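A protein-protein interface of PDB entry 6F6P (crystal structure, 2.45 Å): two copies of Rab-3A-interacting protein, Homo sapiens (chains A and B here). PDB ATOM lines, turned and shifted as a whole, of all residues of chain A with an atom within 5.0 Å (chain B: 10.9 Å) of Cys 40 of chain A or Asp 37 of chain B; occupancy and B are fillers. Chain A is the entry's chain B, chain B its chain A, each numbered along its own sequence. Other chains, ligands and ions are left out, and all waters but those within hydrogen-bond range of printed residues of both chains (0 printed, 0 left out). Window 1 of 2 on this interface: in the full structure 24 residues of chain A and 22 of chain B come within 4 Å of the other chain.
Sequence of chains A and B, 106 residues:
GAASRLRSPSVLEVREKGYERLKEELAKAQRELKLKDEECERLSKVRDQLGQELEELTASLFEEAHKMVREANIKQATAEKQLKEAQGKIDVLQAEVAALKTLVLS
O of Lys 36 of chain B is in hydrogen-bond range of SG of Cys 40 of chain A. The side-chain carboxylate (OD1) of Asp 37 of chain B sits at hydrogen-bond distance from the side-chain sulfur (SG) of Cys 40 of chain A, 3.3 Å away. The backbone carbonyl oxygen (O) of Lys 36 of chain A sits at hydrogen-bond distance from the side-chain sulfur (SG) of Cys 40 of chain B, at 3.4 Å. The side-chain sulfur of Cys 40 of chain B is in hydrogen-bond range of the side-chain carboxylate of Asp 37 of chain A, at 3.4 Å. SG of Cys 40 of chain A lies within hydrogen-bond range of SG of Cys 40 of chain B, at 3.4 Å.
O of Lys 36 of chain B sits at hydrogen-bond distance from SG of Cys 40 of chain B. SG of Cys 40 of chain A sits at hydrogen-bond distance from O of Lys 36 of chain A, 3.5 Å away.
Among the printed residues, merely in contact across the chains: Cys 40 of chain A with Leu 33 of chain B, Lys 36 of chain A with Leu 43 of chain B, Leu 43 of chain A with Glu 32 of chain B, Ser 44 of chain A with Leu 33 of chain B, Leu 43 of chain A with Leu 33 of chain B and Leu 43 of chain A with Lys 36 of chain B.
Of chain B, only Leu 33, Lys 36, Asp 37 and Cys 40 come within 4 Å of Cys 40 of chain A. Of the printed residues of chain A, Asp 37 of chain B touches Cys 40 (3.3 Å). No residue of chain B comes within 4 Å of Glu 39 of chain A. No residue of chain B comes within 4 Å of Glu 41 of chain A. Of chain B, only Glu 32, Leu 33 and Lys 36 come within 4 Å of Leu 43 of chain A. Of chain B, only Leu 33 (3.9 Å) comes within 4 Å of Ser 44 of chain A. Printed residues of chain B within 4 Å of Lys 36 of chain A: Cys 40 and Leu 43. Of the printed residues of chain A, Glu 32 of chain B touches Leu 43. Printed residues of chain B within 4 Å of Asp 37 of chain A: Cys 40 (3.4 Å). The nearest residue of chain B that does not touch Cys 40 of chain A is Glu 38 of chain B (6.0 Å).
Of the 18 printed residues of chain B, 6 touch a printed residue of chain A. Of the 9 printed residues of chain A, 5 touch a printed residue of chain B. Printed residues of chain A that touch a printed residue of chain B: Lys 36, Asp 37, Cys 40, Leu 43 and Ser 44. Hydrophobic or aromatic side chains of chain A within 4 Å of the printed part of chain B: Leu 43. Along chain A the printed residues that touch a printed residue of chain B span positions 36 to 44. Among the printed residues, no Asp or Glu carboxylate lies within 4 Å of a Lys or Arg side-chain nitrogen of the other chain.
Lys 36 of chain A touches Cys 40 of chain B, and with the chains exchanged Cys 40 of chain A touches Lys 36 of chain B. Lys 36 of chain A touches Leu 43 of chain B, and with the chains exchanged Leu 43 of chain A touches Lys 36 of chain B. Asp 37 of chain A touches Cys 40 of chain B, and with the chains exchanged Cys 40 of chain A touches Asp 37 of chain B. Cys 40 of chain A touches its own counterpart, Cys 40 of chain B.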
ATOM      1  N   LYS A  36      -6.535 -21.345   3.010  1.00  0.00           N
ATOM      2  CA  LYS A  36      -7.623 -22.199   3.477  1.00  0.00           C
ATOM      3  C   LYS A  36      -7.651 -23.532   2.738  1.00  0.00           C
ATOM      4  O   LYS A  36      -8.058 -24.548   3.313  1.00  0.00           O
ATOM      5  CB  LYS A  36      -8.959 -21.472   3.331  1.00  0.00           C
ATOM      6  CG  LYS A  36      -8.987 -20.111   4.000  1.00  0.00           C
ATOM      7  CD  LYS A  36      -8.674 -20.200   5.484  1.00  0.00           C
ATOM      8  CE  LYS A  36      -8.592 -18.815   6.104  1.00  0.00           C
ATOM      9  NZ  LYS A  36      -8.385 -18.871   7.577  1.00  0.00           N
ATOM     10  N   ASP A  37      -7.228 -23.550   1.471  1.00  0.00           N
ATOM     11  CA  ASP A  37      -7.137 -24.810   0.738  1.00  0.00           C
ATOM     12  C   ASP A  37      -6.096 -25.732   1.361  1.00  0.00           C
ATOM     13  O   ASP A  37      -6.347 -26.929   1.558  1.00  0.00           O
ATOM     14  CB  ASP A  37      -6.812 -24.543  -0.731  1.00  0.00           C
ATOM     15  CG  ASP A  37      -8.033 -24.144  -1.535  1.00  0.00           C
ATOM     16  OD1 ASP A  37      -9.145 -24.602  -1.194  1.00  0.00           O
ATOM     17  OD2 ASP A  37      -7.883 -23.374  -2.506  1.00  0.00           O
ATOM     18  N   GLU A  38      -4.913 -25.193   1.674  1.00  0.00           N
ATOM     19  CA  GLU A  38      -3.895 -25.999   2.341  1.00  0.00           C
ATOM     20  C   GLU A  38      -4.404 -26.521   3.680  1.00  0.00           C
ATOM     21  O   GLU A  38      -4.167 -27.684   4.037  1.00  0.00           O
ATOM     22  CB  GLU A  38      -2.614 -25.185   2.531  1.00  0.00           C
ATOM     23  CG  GLU A  38      -1.923 -24.801   1.233  1.00  0.00           C
ATOM     24  CD  GLU A  38      -0.787 -23.817   1.444  1.00  0.00           C
ATOM     25  OE1 GLU A  38      -0.688 -23.243   2.549  1.00  0.00           O
ATOM     26  OE2 GLU A  38       0.012 -23.620   0.504  1.00  0.00           O
ATOM     27  N   GLU A  39      -5.121 -25.677   4.426  1.00  0.00           N
ATOM     28  CA  GLU A  39      -5.719 -26.125   5.681  1.00  0.00           C
ATOM     29  C   GLU A  39      -6.693 -27.275   5.448  1.00  0.00           C
ATOM     30  O   GLU A  39      -6.710 -28.250   6.212  1.00  0.00           O
ATOM     31  CB  GLU A  39      -6.417 -24.948   6.364  1.00  0.00           C
ATOM     32  CG  GLU A  39      -7.140 -25.291   7.654  1.00  0.00           C
ATOM     33  CD  GLU A  39      -7.788 -24.074   8.291  1.00  0.00           C
ATOM     34  OE1 GLU A  39      -7.711 -22.978   7.698  1.00  0.00           O
ATOM     35  OE2 GLU A  39      -8.373 -24.215   9.385  1.00  0.00           O
ATOM     36  N   CYS A  40      -7.501 -27.188   4.387  1.00  0.00           N
ATOM     37  CA  CYS A  40      -8.428 -28.271   4.068  1.00  0.00           C
ATOM     38  C   CYS A  40      -7.691 -29.558   3.723  1.00  0.00           C
ATOM     39  O   CYS A  40      -8.145 -30.653   4.074  1.00  0.00           O
ATOM     40  CB  CYS A  40      -9.348 -27.861   2.920  1.00  0.00           C
ATOM     41  SG  CYS A  40     -10.724 -26.814   3.418  1.00  0.00           S
ATOM     42  N   GLU A  41      -6.555 -29.452   3.029  1.00  0.00           N
ATOM     43  CA  GLU A  41      -5.773 -30.648   2.729  1.00  0.00           C
ATOM     44  C   GLU A  41      -5.225 -31.281   4.002  1.00  0.00           C
ATOM     45  O   GLU A  41      -5.284 -32.508   4.169  1.00  0.00           O
ATOM     46  CB  GLU A  41      -4.640 -30.308   1.762  1.00  0.00           C
ATOM     47  CG  GLU A  41      -5.110 -29.951   0.359  1.00  0.00           C
ATOM     48  CD  GLU A  41      -5.845 -31.092  -0.321  1.00  0.00           C
ATOM     49  OE1 GLU A  41      -5.495 -32.264  -0.067  1.00  0.00           O
ATOM     50  OE2 GLU A  41      -6.774 -30.815  -1.109  1.00  0.00           O
ATOM     51  N   ARG A  42      -4.696 -30.460   4.912  1.00  0.00           N
ATOM     52  CA  ARG A  42      -4.204 -30.972   6.188  1.00  0.00           C
ATOM     53  C   ARG A  42      -5.310 -31.689   6.959  1.00  0.00           C
ATOM     54  O   ARG A  42      -5.136 -32.832   7.412  1.00  0.00           O
ATOM     55  CB  ARG A  42      -3.615 -29.818   7.001  1.00  0.00           C
ATOM     56  CG  ARG A  42      -2.947 -30.212   8.304  1.00  0.00           C
ATOM     57  CD  ARG A  42      -2.535 -28.968   9.079  1.00  0.00           C
ATOM     58  NE  ARG A  42      -3.683 -28.176   9.515  1.00  0.00           N
ATOM     59  CZ  ARG A  42      -4.367 -28.398  10.632  1.00  0.00           C
ATOM     60  NH1 ARG A  42      -4.022 -29.393  11.439  1.00  0.00           N
ATOM     61  NH2 ARG A  42      -5.396 -27.622  10.945  1.00  0.00           N
ATOM     62  N   LEU A  43      -6.469 -31.037   7.100  1.00  0.00           N
ATOM     63  CA  LEU A  43      -7.586 -31.656   7.807  1.00  0.00           C
ATOM     64  C   LEU A  43      -8.045 -32.935   7.119  1.00  0.00           C
ATOM     65  O   LEU A  43      -8.456 -33.891   7.790  1.00  0.00           O
ATOM     66  CB  LEU A  43      -8.749 -30.669   7.915  1.00  0.00           C
ATOM     67  CG  LEU A  43      -8.549 -29.454   8.824  1.00  0.00           C
ATOM     68  CD1 LEU A  43      -9.803 -28.595   8.852  1.00  0.00           C
ATOM     69  CD2 LEU A  43      -8.162 -29.891  10.228  1.00  0.00           C
ATOM     70  N   SER A  44      -7.976 -32.976   5.786  1.00  0.00           N
ATOM     71  CA  SER A  44      -8.352 -34.183   5.058  1.00  0.00           C
ATOM     72  C   SER A  44      -7.395 -35.330   5.358  1.00  0.00           C
ATOM     73  O   SER A  44      -7.826 -36.476   5.535  1.00  0.00           O
ATOM     74  CB  SER A  44      -8.397 -33.898   3.558  1.00  0.00           C
ATOM     75  OG  SER A  44      -8.802 -35.046   2.832  1.00  0.00           O
ATOM     76  N   LYS B  28     -15.297 -35.547  14.899  1.00  0.00           N
ATOM     77  CA  LYS B  28     -14.814 -34.181  15.074  1.00  0.00           C
ATOM     78  C   LYS B  28     -13.979 -33.736  13.878  1.00  0.00           C
ATOM     79  O   LYS B  28     -14.166 -32.631  13.347  1.00  0.00           O
ATOM     80  CB  LYS B  28     -13.997 -34.088  16.361  1.00  0.00           C
ATOM     81  CG  LYS B  28     -13.601 -32.680  16.770  1.00  0.00           C
ATOM     82  CD  LYS B  28     -12.881 -32.696  18.110  1.00  0.00           C
ATOM     83  CE  LYS B  28     -12.426 -31.306  18.517  1.00  0.00           C
ATOM     84  NZ  LYS B  28     -11.665 -31.314  19.799  1.00  0.00           N
ATOM     85  N   ALA B  29     -13.055 -34.594  13.430  1.00  0.00           N
ATOM     86  CA  ALA B  29     -12.259 -34.260  12.251  1.00  0.00           C
ATOM     87  C   ALA B  29     -13.138 -34.040  11.025  1.00  0.00           C
ATOM     88  O   ALA B  29     -12.891 -33.126  10.226  1.00  0.00           O
ATOM     89  CB  ALA B  29     -11.231 -35.357  11.982  1.00  0.00           C
ATOM     90  N   GLN B  30     -14.180 -34.861  10.864  1.00  0.00           N
ATOM     91  CA  GLN B  30     -15.085 -34.696   9.730  1.00  0.00           C
ATOM     92  C   GLN B  30     -15.821 -33.364   9.791  1.00  0.00           C
ATOM     93  O   GLN B  30     -15.929 -32.658   8.779  1.00  0.00           O
ATOM     94  CB  GLN B  30     -16.081 -35.855   9.678  1.00  0.00           C
ATOM     95  CG  GLN B  30     -17.059 -35.774   8.518  1.00  0.00           C
ATOM     96  CD  GLN B  30     -18.060 -36.913   8.513  1.00  0.00           C
ATOM     97  OE1 GLN B  30     -18.005 -37.810   9.355  1.00  0.00           O
ATOM     98  NE2 GLN B  30     -18.985 -36.882   7.560  1.00  0.00           N
ATOM     99  N   ARG B  31     -16.331 -32.997  10.970  1.00  0.00           N
ATOM    100  CA  ARG B  31     -17.057 -31.738  11.104  1.00  0.00           C
ATOM    101  C   ARG B  31     -16.151 -30.547  10.805  1.00  0.00           C
ATOM    102  O   ARG B  31     -16.530 -29.634  10.057  1.00  0.00           O
ATOM    103  CB  ARG B  31     -17.664 -31.630  12.503  1.00  0.00           C
ATOM    104  CG  ARG B  31     -18.751 -32.665  12.774  1.00  0.00           C
ATOM    105  CD  ARG B  31     -19.362 -32.521  14.163  1.00  0.00           C
ATOM    106  NE  ARG B  31     -18.431 -32.892  15.226  1.00  0.00           N
ATOM    107  CZ  ARG B  31     -17.876 -32.028  16.070  1.00  0.00           C
ATOM    108  NH1 ARG B  31     -18.158 -30.735  15.981  1.00  0.00           N
ATOM    109  NH2 ARG B  31     -17.042 -32.456  17.007  1.00  0.00           N
ATOM    110  N   GLU B  32     -14.939 -30.548  11.371  1.00  0.00           N
ATOM    111  CA  GLU B  32     -14.012 -29.452  11.103  1.00  0.00           C
ATOM    112  C   GLU B  32     -13.684 -29.366   9.616  1.00  0.00           C
ATOM    113  O   GLU B  32     -13.672 -28.271   9.032  1.00  0.00           O
ATOM    114  CB  GLU B  32     -12.740 -29.616  11.934  1.00  0.00           C
ATOM    115  CG  GLU B  32     -11.895 -28.354  12.018  1.00  0.00           C
ATOM    116  CD  GLU B  32     -10.653 -28.531  12.870  1.00  0.00           C
ATOM    117  OE1 GLU B  32     -10.638 -29.445  13.722  1.00  0.00           O
ATOM    118  OE2 GLU B  32      -9.694 -27.751  12.693  1.00  0.00           O
ATOM    119  N   LEU B  33     -13.429 -30.516   8.982  1.00  0.00           N
ATOM    120  CA  LEU B  33     -13.137 -30.526   7.552  1.00  0.00           C
ATOM    121  C   LEU B  33     -14.295 -29.952   6.744  1.00  0.00           C
ATOM    122  O   LEU B  33     -14.080 -29.203   5.784  1.00  0.00           O
ATOM    123  CB  LEU B  33     -12.816 -31.951   7.094  1.00  0.00           C
ATOM    124  CG  LEU B  33     -12.583 -32.154   5.595  1.00  0.00           C
ATOM    125  CD1 LEU B  33     -11.445 -31.275   5.101  1.00  0.00           C
ATOM    126  CD2 LEU B  33     -12.306 -33.620   5.289  1.00  0.00           C
ATOM    127  N   LYS B  34     -15.533 -30.287   7.120  1.00  0.00           N
ATOM    128  CA  LYS B  34     -16.689 -29.751   6.408  1.00  0.00           C
ATOM    129  C   LYS B  34     -16.776 -28.238   6.562  1.00  0.00           C
ATOM    130  O   LYS B  34     -17.020 -27.517   5.584  1.00  0.00           O
ATOM    131  CB  LYS B  34     -17.971 -30.416   6.909  1.00  0.00           C
ATOM    132  N   LEU B  35     -16.576 -27.737   7.784  1.00  0.00           N
ATOM    133  CA  LEU B  35     -16.596 -26.293   8.004  1.00  0.00           C
ATOM    134  C   LEU B  35     -15.561 -25.591   7.131  1.00  0.00           C
ATOM    135  O   LEU B  35     -15.878 -24.629   6.417  1.00  0.00           O
ATOM    136  CB  LEU B  35     -16.356 -25.988   9.483  1.00  0.00           C
ATOM    137  CG  LEU B  35     -17.523 -26.298  10.424  1.00  0.00           C
ATOM    138  CD1 LEU B  35     -17.092 -26.134  11.872  1.00  0.00           C
ATOM    139  CD2 LEU B  35     -18.720 -25.412  10.111  1.00  0.00           C
ATOM    140  N   LYS B  36     -14.316 -26.073   7.163  1.00  0.00           N
ATOM    141  CA  LYS B  36     -13.270 -25.427   6.375  1.00  0.00           C
ATOM    142  C   LYS B  36     -13.550 -25.531   4.880  1.00  0.00           C
ATOM    143  O   LYS B  36     -13.198 -24.622   4.116  1.00  0.00           O
ATOM    144  CB  LYS B  36     -11.908 -26.036   6.710  1.00  0.00           C
ATOM    145  N   ASP B  37     -14.193 -26.617   4.445  1.00  0.00           N
ATOM    146  CA  ASP B  37     -14.578 -26.733   3.044  1.00  0.00           C
ATOM    147  C   ASP B  37     -15.593 -25.660   2.665  1.00  0.00           C
ATOM    148  O   ASP B  37     -15.467 -25.006   1.621  1.00  0.00           O
ATOM    149  CB  ASP B  37     -15.146 -28.127   2.768  1.00  0.00           C
ATOM    150  CG  ASP B  37     -14.065 -29.170   2.581  1.00  0.00           C
ATOM    151  OD1 ASP B  37     -12.976 -28.812   2.089  1.00  0.00           O
ATOM    152  OD2 ASP B  37     -14.304 -30.346   2.926  1.00  0.00           O
ATOM    153  N   GLU B  38     -16.614 -25.469   3.508  1.00  0.00           N
ATOM    154  CA  GLU B  38     -17.604 -24.430   3.237  1.00  0.00           C
ATOM    155  C   GLU B  38     -16.958 -23.049   3.170  1.00  0.00           C
ATOM    156  O   GLU B  38     -17.284 -22.244   2.283  1.00  0.00           O
ATOM    157  CB  GLU B  38     -18.701 -24.454   4.301  1.00  0.00           C
ATOM    158  CG  GLU B  38     -19.556 -25.714   4.301  1.00  0.00           C
ATOM    159  CD  GLU B  38     -20.480 -25.780   5.501  1.00  0.00           C
ATOM    160  OE1 GLU B  38     -20.277 -24.985   6.440  1.00  0.00           O
ATOM    161  OE2 GLU B  38     -21.405 -26.620   5.502  1.00  0.00           O
ATOM    162  N   GLU B  39     -16.029 -22.758   4.089  1.00  0.00           N
ATOM    163  CA  GLU B  39     -15.321 -21.481   4.015  1.00  0.00           C
ATOM    164  C   GLU B  39     -14.526 -21.360   2.717  1.00  0.00           C
ATOM    165  O   GLU B  39     -14.466 -20.284   2.115  1.00  0.00           O
ATOM    166  CB  GLU B  39     -14.424 -21.282   5.240  1.00  0.00           C
ATOM    167  CG  GLU B  39     -13.627 -19.971   5.215  1.00  0.00           C
ATOM    168  CD  GLU B  39     -14.510 -18.726   5.127  1.00  0.00           C
ATOM    169  OE1 GLU B  39     -15.723 -18.819   5.420  1.00  0.00           O
ATOM    170  OE2 GLU B  39     -13.992 -17.653   4.743  1.00  0.00           O
ATOM    171  N   CYS B  40     -13.906 -22.459   2.271  1.00  0.00           N
ATOM    172  CA  CYS B  40     -13.190 -22.425   0.998  1.00  0.00           C
ATOM    173  C   CYS B  40     -14.129 -22.111  -0.159  1.00  0.00           C
ATOM    174  O   CYS B  40     -13.743 -21.416  -1.106  1.00  0.00           O
ATOM    175  CB  CYS B  40     -12.470 -23.749   0.755  1.00  0.00           C
ATOM    176  SG  CYS B  40     -10.898 -23.905   1.620  1.00  0.00           S
ATOM    177  N   GLU B  41     -15.361 -22.625  -0.112  1.00  0.00           N
ATOM    178  CA  GLU B  41     -16.332 -22.288  -1.151  1.00  0.00           C
ATOM    179  C   GLU B  41     -16.705 -20.810  -1.112  1.00  0.00           C
ATOM    180  O   GLU B  41     -16.766 -20.151  -2.161  1.00  0.00           O
ATOM    181  CB  GLU B  41     -17.578 -23.161  -1.006  1.00  0.00           C
ATOM    182  CG  GLU B  41     -17.351 -24.620  -1.347  1.00  0.00           C
ATOM    183  CD  GLU B  41     -16.933 -24.817  -2.792  1.00  0.00           C
ATOM    184  OE1 GLU B  41     -17.389 -24.042  -3.661  1.00  0.00           O
ATOM    185  OE2 GLU B  41     -16.143 -25.746  -3.061  1.00  0.00           O
ATOM    186  N   ARG B  42     -16.955 -20.268   0.084  1.00  0.00           N
ATOM    187  CA  ARG B  42     -17.282 -18.847   0.194  1.00  0.00           C
ATOM    188  C   ARG B  42     -16.156 -17.974  -0.353  1.00  0.00           C
ATOM    189  O   ARG B  42     -16.387 -17.085  -1.188  1.00  0.00           O
ATOM    190  CB  ARG B  42     -17.584 -18.494   1.650  1.00  0.00           C
ATOM    191  CG  ARG B  42     -18.103 -17.076   1.854  1.00  0.00           C
ATOM    192  CD  ARG B  42     -18.222 -16.724   3.333  1.00  0.00           C
ATOM    193  NE  ARG B  42     -16.925 -16.640   4.000  1.00  0.00           N
ATOM    194  CZ  ARG B  42     -16.166 -15.549   4.013  1.00  0.00           C
ATOM    195  NH1 ARG B  42     -16.575 -14.450   3.394  1.00  0.00           N
ATOM    196  NH2 ARG B  42     -15.000 -15.553   4.646  1.00  0.00           N
ATOM    197  N   LEU B  43     -14.924 -18.218   0.107  1.00  0.00           N
ATOM    198  CA  LEU B  43     -13.785 -17.443  -0.372  1.00  0.00           C
ATOM    199  C   LEU B  43     -13.574 -17.623  -1.869  1.00  0.00           C
ATOM    200  O   LEU B  43     -13.130 -16.691  -2.551  1.00  0.00           O
ATOM    201  CB  LEU B  43     -12.530 -17.836   0.399  1.00  0.00           C
ATOM    202  CG  LEU B  43     -12.538 -17.415   1.868  1.00  0.00           C
ATOM    203  CD1 LEU B  43     -11.245 -17.819   2.533  1.00  0.00           C
ATOM    204  CD2 LEU B  43     -12.766 -15.915   2.012  1.00  0.00           C
ATOM    205  N   SER B  44     -13.874 -18.813  -2.393  1.00  0.00           N
ATOM    206  CA  SER B  44     -13.762 -19.035  -3.831  1.00  0.00           C
ATOM    207  C   SER B  44     -14.762 -18.176  -4.593  1.00  0.00           C
ATOM    208  O   SER B  44     -14.432 -17.612  -5.644  1.00  0.00           O
ATOM    209  CB  SER B  44     -13.966 -20.516  -4.148  1.00  0.00           C
ATOM    210  OG  SER B  44     -13.821 -20.766  -5.534  1.00  0.00           O
ATOM    211  N   LYS B  45     -15.989 -18.064  -4.077  1.00  0.00           N
ATOM    212  CA  LYS B  45     -16.981 -17.204  -4.718  1.00  0.00           C
ATOM    213  C   LYS B  45     -16.550 -15.743  -4.673  1.00  0.00           C
ATOM    214  O   LYS B  45     -16.704 -15.012  -5.661  1.00  0.00           O
ATOM    215  CB  LYS B  45     -18.344 -17.387  -4.051  1.00  0.00           C
ATOM    216  CG  LYS B  45     -18.917 -18.789  -4.195  1.00  0.00           C
ATOM    217  CD  LYS B  45     -20.237 -18.934  -3.454  1.00  0.00           C
ATOM    218  CE  LYS B  45     -20.749 -20.365  -3.521  1.00  0.00           C
ATOM    219  NZ  LYS B  45     -22.007 -20.548  -2.746  1.00  0.00           N
